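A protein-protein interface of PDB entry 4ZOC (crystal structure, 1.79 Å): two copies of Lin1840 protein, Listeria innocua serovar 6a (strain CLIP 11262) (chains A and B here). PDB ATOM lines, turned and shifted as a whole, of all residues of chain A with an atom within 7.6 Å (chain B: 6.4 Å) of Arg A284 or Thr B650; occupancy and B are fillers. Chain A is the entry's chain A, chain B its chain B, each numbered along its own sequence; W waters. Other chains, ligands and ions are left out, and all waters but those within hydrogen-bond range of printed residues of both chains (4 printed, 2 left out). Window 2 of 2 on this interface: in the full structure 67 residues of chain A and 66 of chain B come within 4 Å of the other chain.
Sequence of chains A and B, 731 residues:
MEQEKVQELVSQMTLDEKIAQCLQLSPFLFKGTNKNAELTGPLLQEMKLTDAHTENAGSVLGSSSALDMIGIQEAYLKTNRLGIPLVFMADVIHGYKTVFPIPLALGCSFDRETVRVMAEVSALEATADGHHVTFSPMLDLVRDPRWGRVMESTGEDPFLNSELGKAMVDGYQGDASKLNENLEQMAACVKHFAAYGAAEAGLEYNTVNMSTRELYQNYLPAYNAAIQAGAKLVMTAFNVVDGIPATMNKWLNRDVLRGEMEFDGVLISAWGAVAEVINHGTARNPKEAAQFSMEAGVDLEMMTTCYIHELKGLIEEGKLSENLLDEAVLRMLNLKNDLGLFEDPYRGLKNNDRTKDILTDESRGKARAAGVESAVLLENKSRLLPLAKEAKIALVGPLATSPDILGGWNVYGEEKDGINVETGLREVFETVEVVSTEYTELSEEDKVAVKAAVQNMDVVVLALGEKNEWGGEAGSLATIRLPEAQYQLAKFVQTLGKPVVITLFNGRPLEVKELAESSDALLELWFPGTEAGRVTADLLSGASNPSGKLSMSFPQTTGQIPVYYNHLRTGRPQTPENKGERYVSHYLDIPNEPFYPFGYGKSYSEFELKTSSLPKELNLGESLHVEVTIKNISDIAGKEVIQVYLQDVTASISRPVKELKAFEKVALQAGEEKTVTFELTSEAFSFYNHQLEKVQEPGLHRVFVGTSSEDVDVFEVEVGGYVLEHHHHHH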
ATOM      1  N   VAL A 277     -26.896   9.111  -6.952  1.00  0.00           N
ATOM      2  CA  VAL A 277     -27.305   7.718  -7.244  1.00  0.00           C
ATOM      3  C   VAL A 277     -27.273   6.922  -5.920  1.00  0.00           C
ATOM      4  O   VAL A 277     -28.001   5.881  -5.755  1.00  0.00           O
ATOM      5  CB  VAL A 277     -26.537   7.058  -8.416  1.00  0.00           C
ATOM      6  CG1 VAL A 277     -26.546   7.887  -9.659  1.00  0.00           C
ATOM      7  CG2 VAL A 277     -25.100   6.713  -8.083  1.00  0.00           C
ATOM      8  N   ILE A 278     -26.452   7.378  -4.974  1.00  0.00           N
ATOM      9  CA  ILE A 278     -26.505   6.831  -3.602  1.00  0.00           C
ATOM     10  C   ILE A 278     -27.896   7.001  -2.930  1.00  0.00           C
ATOM     11  O   ILE A 278     -28.441   6.064  -2.319  1.00  0.00           O
ATOM     12  CB  ILE A 278     -25.362   7.431  -2.725  1.00  0.00           C
ATOM     13  CG1 ILE A 278     -23.999   7.144  -3.379  1.00  0.00           C
ATOM     14  CG2 ILE A 278     -25.429   6.773  -1.358  1.00  0.00           C
ATOM     15  CD1 ILE A 278     -22.901   8.004  -2.767  1.00  0.00           C
ATOM     16  N   ASN A 279     -28.427   8.220  -2.963  1.00  0.00           N
ATOM     17  CA  ASN A 279     -29.710   8.489  -2.404  1.00  0.00           C
ATOM     18  C   ASN A 279     -30.830   7.636  -3.028  1.00  0.00           C
ATOM     19  O   ASN A 279     -31.748   7.230  -2.329  1.00  0.00           O
ATOM     20  CB  ASN A 279     -30.080   9.950  -2.499  1.00  0.00           C
ATOM     21  CG  ASN A 279     -29.202  10.829  -1.653  1.00  0.00           C
ATOM     22  OD1 ASN A 279     -28.697  10.410  -0.593  1.00  0.00           O
ATOM     23  ND2 ASN A 279     -29.130  12.115  -2.017  1.00  0.00           N
ATOM     24  N   HIS A 280     -30.779   7.451  -4.351  1.00  0.00           N
ATOM     25  CA  HIS A 280     -31.680   6.586  -5.087  1.00  0.00           C
ATOM     26  C   HIS A 280     -31.564   5.126  -4.640  1.00  0.00           C
ATOM     27  O   HIS A 280     -32.450   4.302  -4.949  1.00  0.00           O
ATOM     28  CB  HIS A 280     -31.327   6.627  -6.604  1.00  0.00           C
ATOM     29  CG  HIS A 280     -31.824   7.782  -7.409  1.00  0.00           C
ATOM     30  ND1 HIS A 280     -33.143   7.898  -7.779  1.00  0.00           N
ATOM     31  CD2 HIS A 280     -31.147   8.764  -8.077  1.00  0.00           C
ATOM     32  CE1 HIS A 280     -33.262   8.926  -8.610  1.00  0.00           C
ATOM     33  NE2 HIS A 280     -32.065   9.469  -8.820  1.00  0.00           N
ATOM     34  N   GLY A 281     -30.479   4.735  -4.007  1.00  0.00           N
ATOM     35  CA  GLY A 281     -30.327   3.351  -3.532  1.00  0.00           C
ATOM     36  C   GLY A 281     -29.834   2.367  -4.546  1.00  0.00           C
ATOM     37  O   GLY A 281     -30.176   1.150  -4.476  1.00  0.00           O
ATOM     38  N   THR A 282     -29.065   2.890  -5.522  1.00  0.00           N
ATOM     39  CA  THR A 282     -28.461   2.028  -6.534  1.00  0.00           C
ATOM     40  C   THR A 282     -26.892   2.089  -6.476  1.00  0.00           C
ATOM     41  O   THR A 282     -26.217   1.552  -7.345  1.00  0.00           O
ATOM     42  CB  THR A 282     -28.987   2.344  -7.940  1.00  0.00           C
ATOM     43  OG1 THR A 282     -28.728   3.747  -8.244  1.00  0.00           O
ATOM     44  CG2 THR A 282     -30.513   2.064  -8.043  1.00  0.00           C
ATOM     45  N   ALA A 283     -26.340   2.740  -5.467  1.00  0.00           N
ATOM     46  CA  ALA A 283     -24.919   2.641  -5.191  1.00  0.00           C
ATOM     47  C   ALA A 283     -24.820   2.780  -3.678  1.00  0.00           C
ATOM     48  O   ALA A 283     -25.494   3.595  -3.072  1.00  0.00           O
ATOM     49  CB  ALA A 283     -24.111   3.701  -5.898  1.00  0.00           C
ATOM     50  N   ARG A 284     -23.919   2.017  -3.056  1.00  0.00           N
ATOM     51  CA  ARG A 284     -23.859   2.020  -1.575  1.00  0.00           C
ATOM     52  C   ARG A 284     -23.063   3.202  -1.018  1.00  0.00           C
ATOM     53  O   ARG A 284     -23.268   3.645   0.085  1.00  0.00           O
ATOM     54  CB  ARG A 284     -23.278   0.633  -1.062  1.00  0.00           C
ATOM     55  CG  ARG A 284     -23.311   0.411   0.483  1.00  0.00           C
ATOM     56  CD  ARG A 284     -22.933  -1.048   0.848  1.00  0.00           C
ATOM     57  NE  ARG A 284     -23.364  -1.413   2.217  1.00  0.00           N
ATOM     58  CZ  ARG A 284     -23.651  -2.662   2.700  1.00  0.00           C
ATOM     59  NH1 ARG A 284     -24.023  -2.834   3.973  1.00  0.00           N
ATOM     60  NH2 ARG A 284     -23.572  -3.779   1.966  1.00  0.00           N
ATOM     61  N   ASN A 285     -22.182   3.731  -1.806  1.00  0.00           N
ATOM     62  CA  ASN A 285     -21.214   4.751  -1.306  1.00  0.00           C
ATOM     63  C   ASN A 285     -20.635   5.499  -2.496  1.00  0.00           C
ATOM     64  O   ASN A 285     -20.900   5.120  -3.669  1.00  0.00           O
ATOM     65  CB  ASN A 285     -20.113   4.072  -0.479  1.00  0.00           C
ATOM     66  CG  ASN A 285     -19.469   2.896  -1.209  1.00  0.00           C
ATOM     67  OD1 ASN A 285     -19.229   2.934  -2.399  1.00  0.00           O
ATOM     68  ND2 ASN A 285     -19.214   1.830  -0.481  1.00  0.00           N
ATOM     69  N   PRO A 286     -19.826   6.554  -2.242  1.00  0.00           N
ATOM     70  CA  PRO A 286     -19.175   7.267  -3.369  1.00  0.00           C
ATOM     71  C   PRO A 286     -18.335   6.433  -4.300  1.00  0.00           C
ATOM     72  O   PRO A 286     -18.178   6.763  -5.464  1.00  0.00           O
ATOM     73  CB  PRO A 286     -18.371   8.367  -2.670  1.00  0.00           C
ATOM     74  CG  PRO A 286     -19.132   8.597  -1.427  1.00  0.00           C
ATOM     75  CD  PRO A 286     -19.597   7.229  -0.981  1.00  0.00           C
ATOM     76  N   LYS A 287     -17.746   5.352  -3.796  1.00  0.00           N
ATOM     77  CA  LYS A 287     -16.901   4.507  -4.624  1.00  0.00           C
ATOM     78  C   LYS A 287     -17.738   3.764  -5.678  1.00  0.00           C
ATOM     79  O   LYS A 287     -17.410   3.720  -6.827  1.00  0.00           O
ATOM     80  CB  LYS A 287     -16.140   3.516  -3.696  1.00  0.00           C
ATOM     81  CG  LYS A 287     -15.199   2.584  -4.427  1.00  0.00           C
ATOM     82  CD  LYS A 287     -14.435   1.727  -3.427  1.00  0.00           C
ATOM     83  CE  LYS A 287     -13.352   0.957  -4.156  1.00  0.00           C
ATOM     84  NZ  LYS A 287     -12.646   0.162  -3.139  1.00  0.00           N
ATOM     85  N   GLU A 288     -18.890   3.253  -5.262  1.00  0.00           N
ATOM     86  CA  GLU A 288     -19.754   2.653  -6.219  1.00  0.00           C
ATOM     87  C   GLU A 288     -20.376   3.667  -7.214  1.00  0.00           C
ATOM     88  O   GLU A 288     -20.517   3.371  -8.390  1.00  0.00           O
ATOM     89  CB  GLU A 288     -20.880   1.854  -5.472  1.00  0.00           C
ATOM     90  CG  GLU A 288     -20.326   0.568  -4.806  1.00  0.00           C
ATOM     91  CD  GLU A 288     -21.378  -0.431  -4.384  1.00  0.00           C
ATOM     92  OE1 GLU A 288     -22.619  -0.152  -4.446  1.00  0.00           O
ATOM     93  OE2 GLU A 288     -20.951  -1.502  -3.901  1.00  0.00           O
ATOM     94  N   ALA A 289     -20.792   4.820  -6.697  1.00  0.00           N
ATOM     95  CA  ALA A 289     -21.332   5.902  -7.527  1.00  0.00           C
ATOM     96  C   ALA A 289     -20.366   6.262  -8.660  1.00  0.00           C
ATOM     97  O   ALA A 289     -20.737   6.319  -9.846  1.00  0.00           O
ATOM     98  CB  ALA A 289     -21.627   7.128  -6.685  1.00  0.00           C
ATOM     99  N   PHE A 292     -20.024   3.083 -11.162  1.00  0.00           N
ATOM    100  CA  PHE A 292     -21.189   2.822 -12.040  1.00  0.00           C
ATOM    101  C   PHE A 292     -21.399   4.001 -13.013  1.00  0.00           C
ATOM    102  O   PHE A 292     -21.707   3.806 -14.146  1.00  0.00           O
ATOM    103  CB  PHE A 292     -22.448   2.556 -11.194  1.00  0.00           C
ATOM    104  CG  PHE A 292     -22.303   1.441 -10.187  1.00  0.00           C
ATOM    105  CD1 PHE A 292     -21.412   0.389 -10.407  1.00  0.00           C
ATOM    106  CD2 PHE A 292     -23.106   1.405  -9.071  1.00  0.00           C
ATOM    107  CE1 PHE A 292     -21.321  -0.637  -9.467  1.00  0.00           C
ATOM    108  CE2 PHE A 292     -23.033   0.352  -8.148  1.00  0.00           C
ATOM    109  CZ  PHE A 292     -22.130  -0.641  -8.367  1.00  0.00           C
ATOM    110  N   ASP B 648     -34.940  -2.874   0.794  1.00  0.00           N
ATOM    111  CA  ASP B 648     -33.671  -3.221   0.167  1.00  0.00           C
ATOM    112  C   ASP B 648     -32.910  -1.923   0.037  1.00  0.00           C
ATOM    113  O   ASP B 648     -33.198  -1.132  -0.812  1.00  0.00           O
ATOM    114  CB  ASP B 648     -33.915  -3.934  -1.151  1.00  0.00           C
ATOM    115  CG  ASP B 648     -32.683  -4.533  -1.758  1.00  0.00           C
ATOM    116  OD1 ASP B 648     -31.531  -4.299  -1.319  1.00  0.00           O
ATOM    117  OD2 ASP B 648     -32.902  -5.336  -2.743  1.00  0.00           O
ATOM    118  N   VAL B 649     -31.873  -1.741   0.850  1.00  0.00           N
ATOM    119  CA  VAL B 649     -31.226  -0.423   0.944  1.00  0.00           C
ATOM    120  C   VAL B 649     -30.508  -0.015  -0.359  1.00  0.00           C
ATOM    121  O   VAL B 649     -30.560   1.142  -0.811  1.00  0.00           O
ATOM    122  CB  VAL B 649     -30.357  -0.294   2.178  1.00  0.00           C
ATOM    123  CG1 VAL B 649     -29.638   1.013   2.218  1.00  0.00           C
ATOM    124  CG2 VAL B 649     -31.190  -0.508   3.434  1.00  0.00           C
ATOM    125  N   THR B 650     -29.806  -0.938  -0.946  1.00  0.00           N
ATOM    126  CA  THR B 650     -29.078  -0.669  -2.197  1.00  0.00           C
ATOM    127  C   THR B 650     -29.315  -1.810  -3.152  1.00  0.00           C
ATOM    128  O   THR B 650     -29.248  -2.953  -2.739  1.00  0.00           O
ATOM    129  CB  THR B 650     -27.566  -0.523  -1.924  1.00  0.00           C
ATOM    130  OG1 THR B 650     -27.339   0.424  -0.893  1.00  0.00           O
ATOM    131  CG2 THR B 650     -26.802  -0.175  -3.172  1.00  0.00           C
ATOM    132  N   ALA B 651     -29.592  -1.532  -4.417  1.00  0.00           N
ATOM    133  CA  ALA B 651     -29.887  -2.586  -5.327  1.00  0.00           C
ATOM    134  C   ALA B 651     -29.595  -2.155  -6.733  1.00  0.00           C
ATOM    135  O   ALA B 651     -29.384  -0.977  -6.984  1.00  0.00           O
ATOM    136  CB  ALA B 651     -31.363  -3.037  -5.189  1.00  0.00           C
ATOM    137  N   SER B 652     -29.548  -3.106  -7.644  1.00  0.00           N
ATOM    138  CA  SER B 652     -29.384  -2.787  -9.072  1.00  0.00           C
ATOM    139  C   SER B 652     -30.573  -2.081  -9.731  1.00  0.00           C
ATOM    140  O   SER B 652     -30.429  -1.596 -10.827  1.00  0.00           O
ATOM    141  CB  SER B 652     -29.027  -4.001  -9.880  1.00  0.00           C
ATOM    142  OG  SER B 652     -30.064  -4.952  -9.863  1.00  0.00           O
ATOM    143  N   ILE B 653     -31.707  -2.042  -9.025  1.00  0.00           N
ATOM    144  CA  ILE B 653     -32.898  -1.228  -9.369  1.00  0.00           C
ATOM    145  C   ILE B 653     -33.189  -0.406  -8.078  1.00  0.00           C
ATOM    146  O   ILE B 653     -33.069  -0.911  -6.995  1.00  0.00           O
ATOM    147  CB  ILE B 653     -34.077  -2.185  -9.705  1.00  0.00           C
ATOM    148  CG1 ILE B 653     -33.796  -3.025 -11.021  1.00  0.00           C
ATOM    149  CG2 ILE B 653     -35.398  -1.432  -9.722  1.00  0.00           C
ATOM    150  CD1 ILE B 653     -33.717  -2.185 -12.264  1.00  0.00           C
ATOM    151  N   ARG B 655     -35.153   0.594  -5.208  1.00  0.00           N
ATOM    152  CA  ARG B 655     -36.248  -0.163  -4.607  1.00  0.00           C
ATOM    153  C   ARG B 655     -37.091   0.698  -3.655  1.00  0.00           C
ATOM    154  O   ARG B 655     -36.595   1.675  -3.083  1.00  0.00           O
ATOM    155  CB  ARG B 655     -35.710  -1.402  -3.851  1.00  0.00           C
ATOM    156  CG  ARG B 655     -34.926  -2.380  -4.663  1.00  0.00           C
ATOM    157  CD  ARG B 655     -35.809  -3.362  -5.421  1.00  0.00           C
ATOM    158  NE  ARG B 655     -36.347  -4.254  -4.528  1.00  0.00           N
ATOM    159  CZ  ARG B 655     -37.640  -4.495  -4.212  1.00  0.00           C
ATOM    160  NH1 ARG B 655     -37.760  -5.250  -3.197  1.00  0.00           N
ATOM    161  NH2 ARG B 655     -38.788  -4.054  -4.806  1.00  0.00           N
ATOM    162  N   GLU B 697     -30.145 -10.252  -4.219  1.00  0.00           N
ATOM    163  CA  GLU B 697     -28.783  -9.730  -4.243  1.00  0.00           C
ATOM    164  C   GLU B 697     -28.324  -9.640  -2.804  1.00  0.00           C
ATOM    165  O   GLU B 697     -29.077  -9.240  -1.935  1.00  0.00           O
ATOM    166  CB  GLU B 697     -28.709  -8.308  -4.878  1.00  0.00           C
ATOM    167  CG  GLU B 697     -29.212  -8.273  -6.316  1.00  0.00           C
ATOM    168  CD  GLU B 697     -29.284  -6.887  -6.895  1.00  0.00           C
ATOM    169  OE1 GLU B 697     -29.444  -5.900  -6.112  1.00  0.00           O
ATOM    170  OE2 GLU B 697     -29.232  -6.818  -8.131  1.00  0.00           O
ATOM    171  N   PRO B 698     -27.046  -9.944  -2.561  1.00  0.00           N
ATOM    172  CA  PRO B 698     -26.486  -9.681  -1.229  1.00  0.00           C
ATOM    173  C   PRO B 698     -26.488  -8.191  -0.937  1.00  0.00           C
ATOM    174  O   PRO B 698     -26.305  -7.379  -1.886  1.00  0.00           O
ATOM    175  CB  PRO B 698     -25.048 -10.262  -1.297  1.00  0.00           C
ATOM    176  CG  PRO B 698     -24.759 -10.387  -2.734  1.00  0.00           C
ATOM    177  CD  PRO B 698     -26.043 -10.405  -3.526  1.00  0.00           C
ATOM    178  N   GLY B 699     -26.612  -7.890   0.368  1.00  0.00           N
ATOM    179  CA  GLY B 699     -26.629  -6.554   0.842  1.00  0.00           C
ATOM    180  C   GLY B 699     -27.458  -6.333   2.079  1.00  0.00           C
ATOM    181  O   GLY B 699     -27.999  -7.299   2.674  1.00  0.00           O
ATOM    182  N   LEU B 700     -27.559  -5.034   2.434  1.00  0.00           N
ATOM    183  CA  LEU B 700     -28.290  -4.616   3.604  1.00  0.00           C
ATOM    184  C   LEU B 700     -29.780  -4.497   3.332  1.00  0.00           C
ATOM    185  O   LEU B 700     -30.193  -3.905   2.315  1.00  0.00           O
ATOM    186  CB  LEU B 700     -27.786  -3.258   4.042  1.00  0.00           C
ATOM    187  CG  LEU B 700     -28.287  -2.615   5.351  1.00  0.00           C
ATOM    188  CD1 LEU B 700     -27.955  -3.444   6.584  1.00  0.00           C
ATOM    189  CD2 LEU B 700     -27.787  -1.161   5.491  1.00  0.00           C
ATOM    190  N   HIS B 701     -30.557  -4.991   4.277  1.00  0.00           N
ATOM    191  CA  HIS B 701     -32.005  -4.842   4.294  1.00  0.00           C
ATOM    192  C   HIS B 701     -32.370  -4.250   5.651  1.00  0.00           C
ATOM    193  O   HIS B 701     -31.655  -4.481   6.659  1.00  0.00           O
ATOM    194  CB  HIS B 701     -32.693  -6.192   4.033  1.00  0.00           C
ATOM    195  CG  HIS B 701     -32.559  -6.654   2.615  1.00  0.00           C
ATOM    196  ND1 HIS B 701     -33.584  -6.585   1.679  1.00  0.00           N
ATOM    197  CD2 HIS B 701     -31.506  -7.194   1.980  1.00  0.00           C
ATOM    198  CE1 HIS B 701     -33.156  -7.079   0.543  1.00  0.00           C
ATOM    199  NE2 HIS B 701     -31.900  -7.464   0.706  1.00  0.00           N
ATOM    200  N   GLU B 718     -27.825  -7.967   7.260  1.00  0.00           N
ATOM    201  CA  GLU B 718     -26.935  -8.004   6.192  1.00  0.00           C
ATOM    202  C   GLU B 718     -26.988  -9.416   5.597  1.00  0.00           C
ATOM    203  O   GLU B 718     -26.635 -10.426   6.264  1.00  0.00           O
ATOM    204  CB  GLU B 718     -25.528  -7.578   6.662  1.00  0.00           C
ATOM    205  CG  GLU B 718     -24.531  -7.433   5.505  1.00  0.00           C
ATOM    206  CD  GLU B 718     -24.652  -6.186   4.587  1.00  0.00           C
ATOM    207  OE1 GLU B 718     -24.919  -5.065   5.048  1.00  0.00           O
ATOM    208  OE2 GLU B 718     -24.313  -6.322   3.394  1.00  0.00           O
HETATM  209  O   HOH W   1     -26.459  -3.180   0.517  1.00  0.00           O
HETATM  210  O   HOH W   2     -35.553   3.981  -3.801  1.00  0.00           O
HETATM  211  O   HOH W   3     -26.482  -0.953  -8.418  1.00  0.00           O
HETATM  212  O   HOH W   4     -26.720  -0.678   1.548  1.00  0.00           O
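Of the 13 printed residues of chain B, 6 touch a printed residue of chain A.
Hydrophobic or aromatic side chains of chain B within 4 Å of the printed part of chain A: Leu B700.
Among the printed residues, Asp or Glu carboxylates within 4 Å of a Lys or Arg side-chain nitrogen of the other chain: Arg A284 with Glu B718.
Water W2 bridges the backbone carbonyl oxygen of Arg B655 and the backbone carbonyl oxygen of His A280.
Water W3 lies within hydrogen-bond range of O of Thr A282 and O of Ala B651.
Water W1 bridges the backbone NH (N) of Leu B700 (2.9 Å) and the guanidinium group (NH2) of Arg A284 (3.3 Å).
The guanidinium group (NH1) of Arg A284 lies within salt-bridge range of the side-chain carboxylate (OE1) of Glu B718.
O of Gly A281 sits at hydrogen-bond distance from N of Ala B651, 2.7 Å away.
Of the printed residues of chain B, Gly A281 touches Val B649, Thr B650 and Ala B651.
Of the printed residues of chain B, Thr A282 touches Ala B651 (3.2 Å) and Ile B653 (3.6 Å).
Of the printed residues of chain B, Ala A283 touches Thr B650.
Lys A287 touches none of the printed residues of chain B.
Of the printed residues of chain A, Val B649 touches Gly A281.
Printed residues of chain A within 4 Å of Thr B650: Gly A281 (3.1 Å), Ala A283 (3.6 Å) and Arg A284 (3.6 Å).
Of the printed residues of chain A, Ile B653 touches Thr A282.
The nearest printed residue of chain A that does not touch Thr B650 is Thr A282 (4.01 Å).
No position is printed for both chains.
Of the 9 pairs that touch across the chains among the printed residues, none has its exchanged pair printed and touching as well.
Gly A281 touches Val B649 (CA to O, 3.5 Å).
Gly A281 touches Thr B650.
CA of Thr A282 touches O of Ala B651, 3.2 Å away.
Ile B653 touches Thr A282.
Thr B650 touches Ala A283.
Thr B650 touches Arg A284.
Leu B700 touches Arg A284.
The backbone NH of Val B649 lies within hydrogen-bond range of the backbone carbonyl oxygen of Leu B700 (3.1 Å).
The backbone NH of Arg A284 lies within hydrogen-bond range of the side-chain carboxylate of Glu A288 (2.9 Å).
O of Val A277 is in hydrogen-bond range of N of Thr A282 (3.2 Å).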
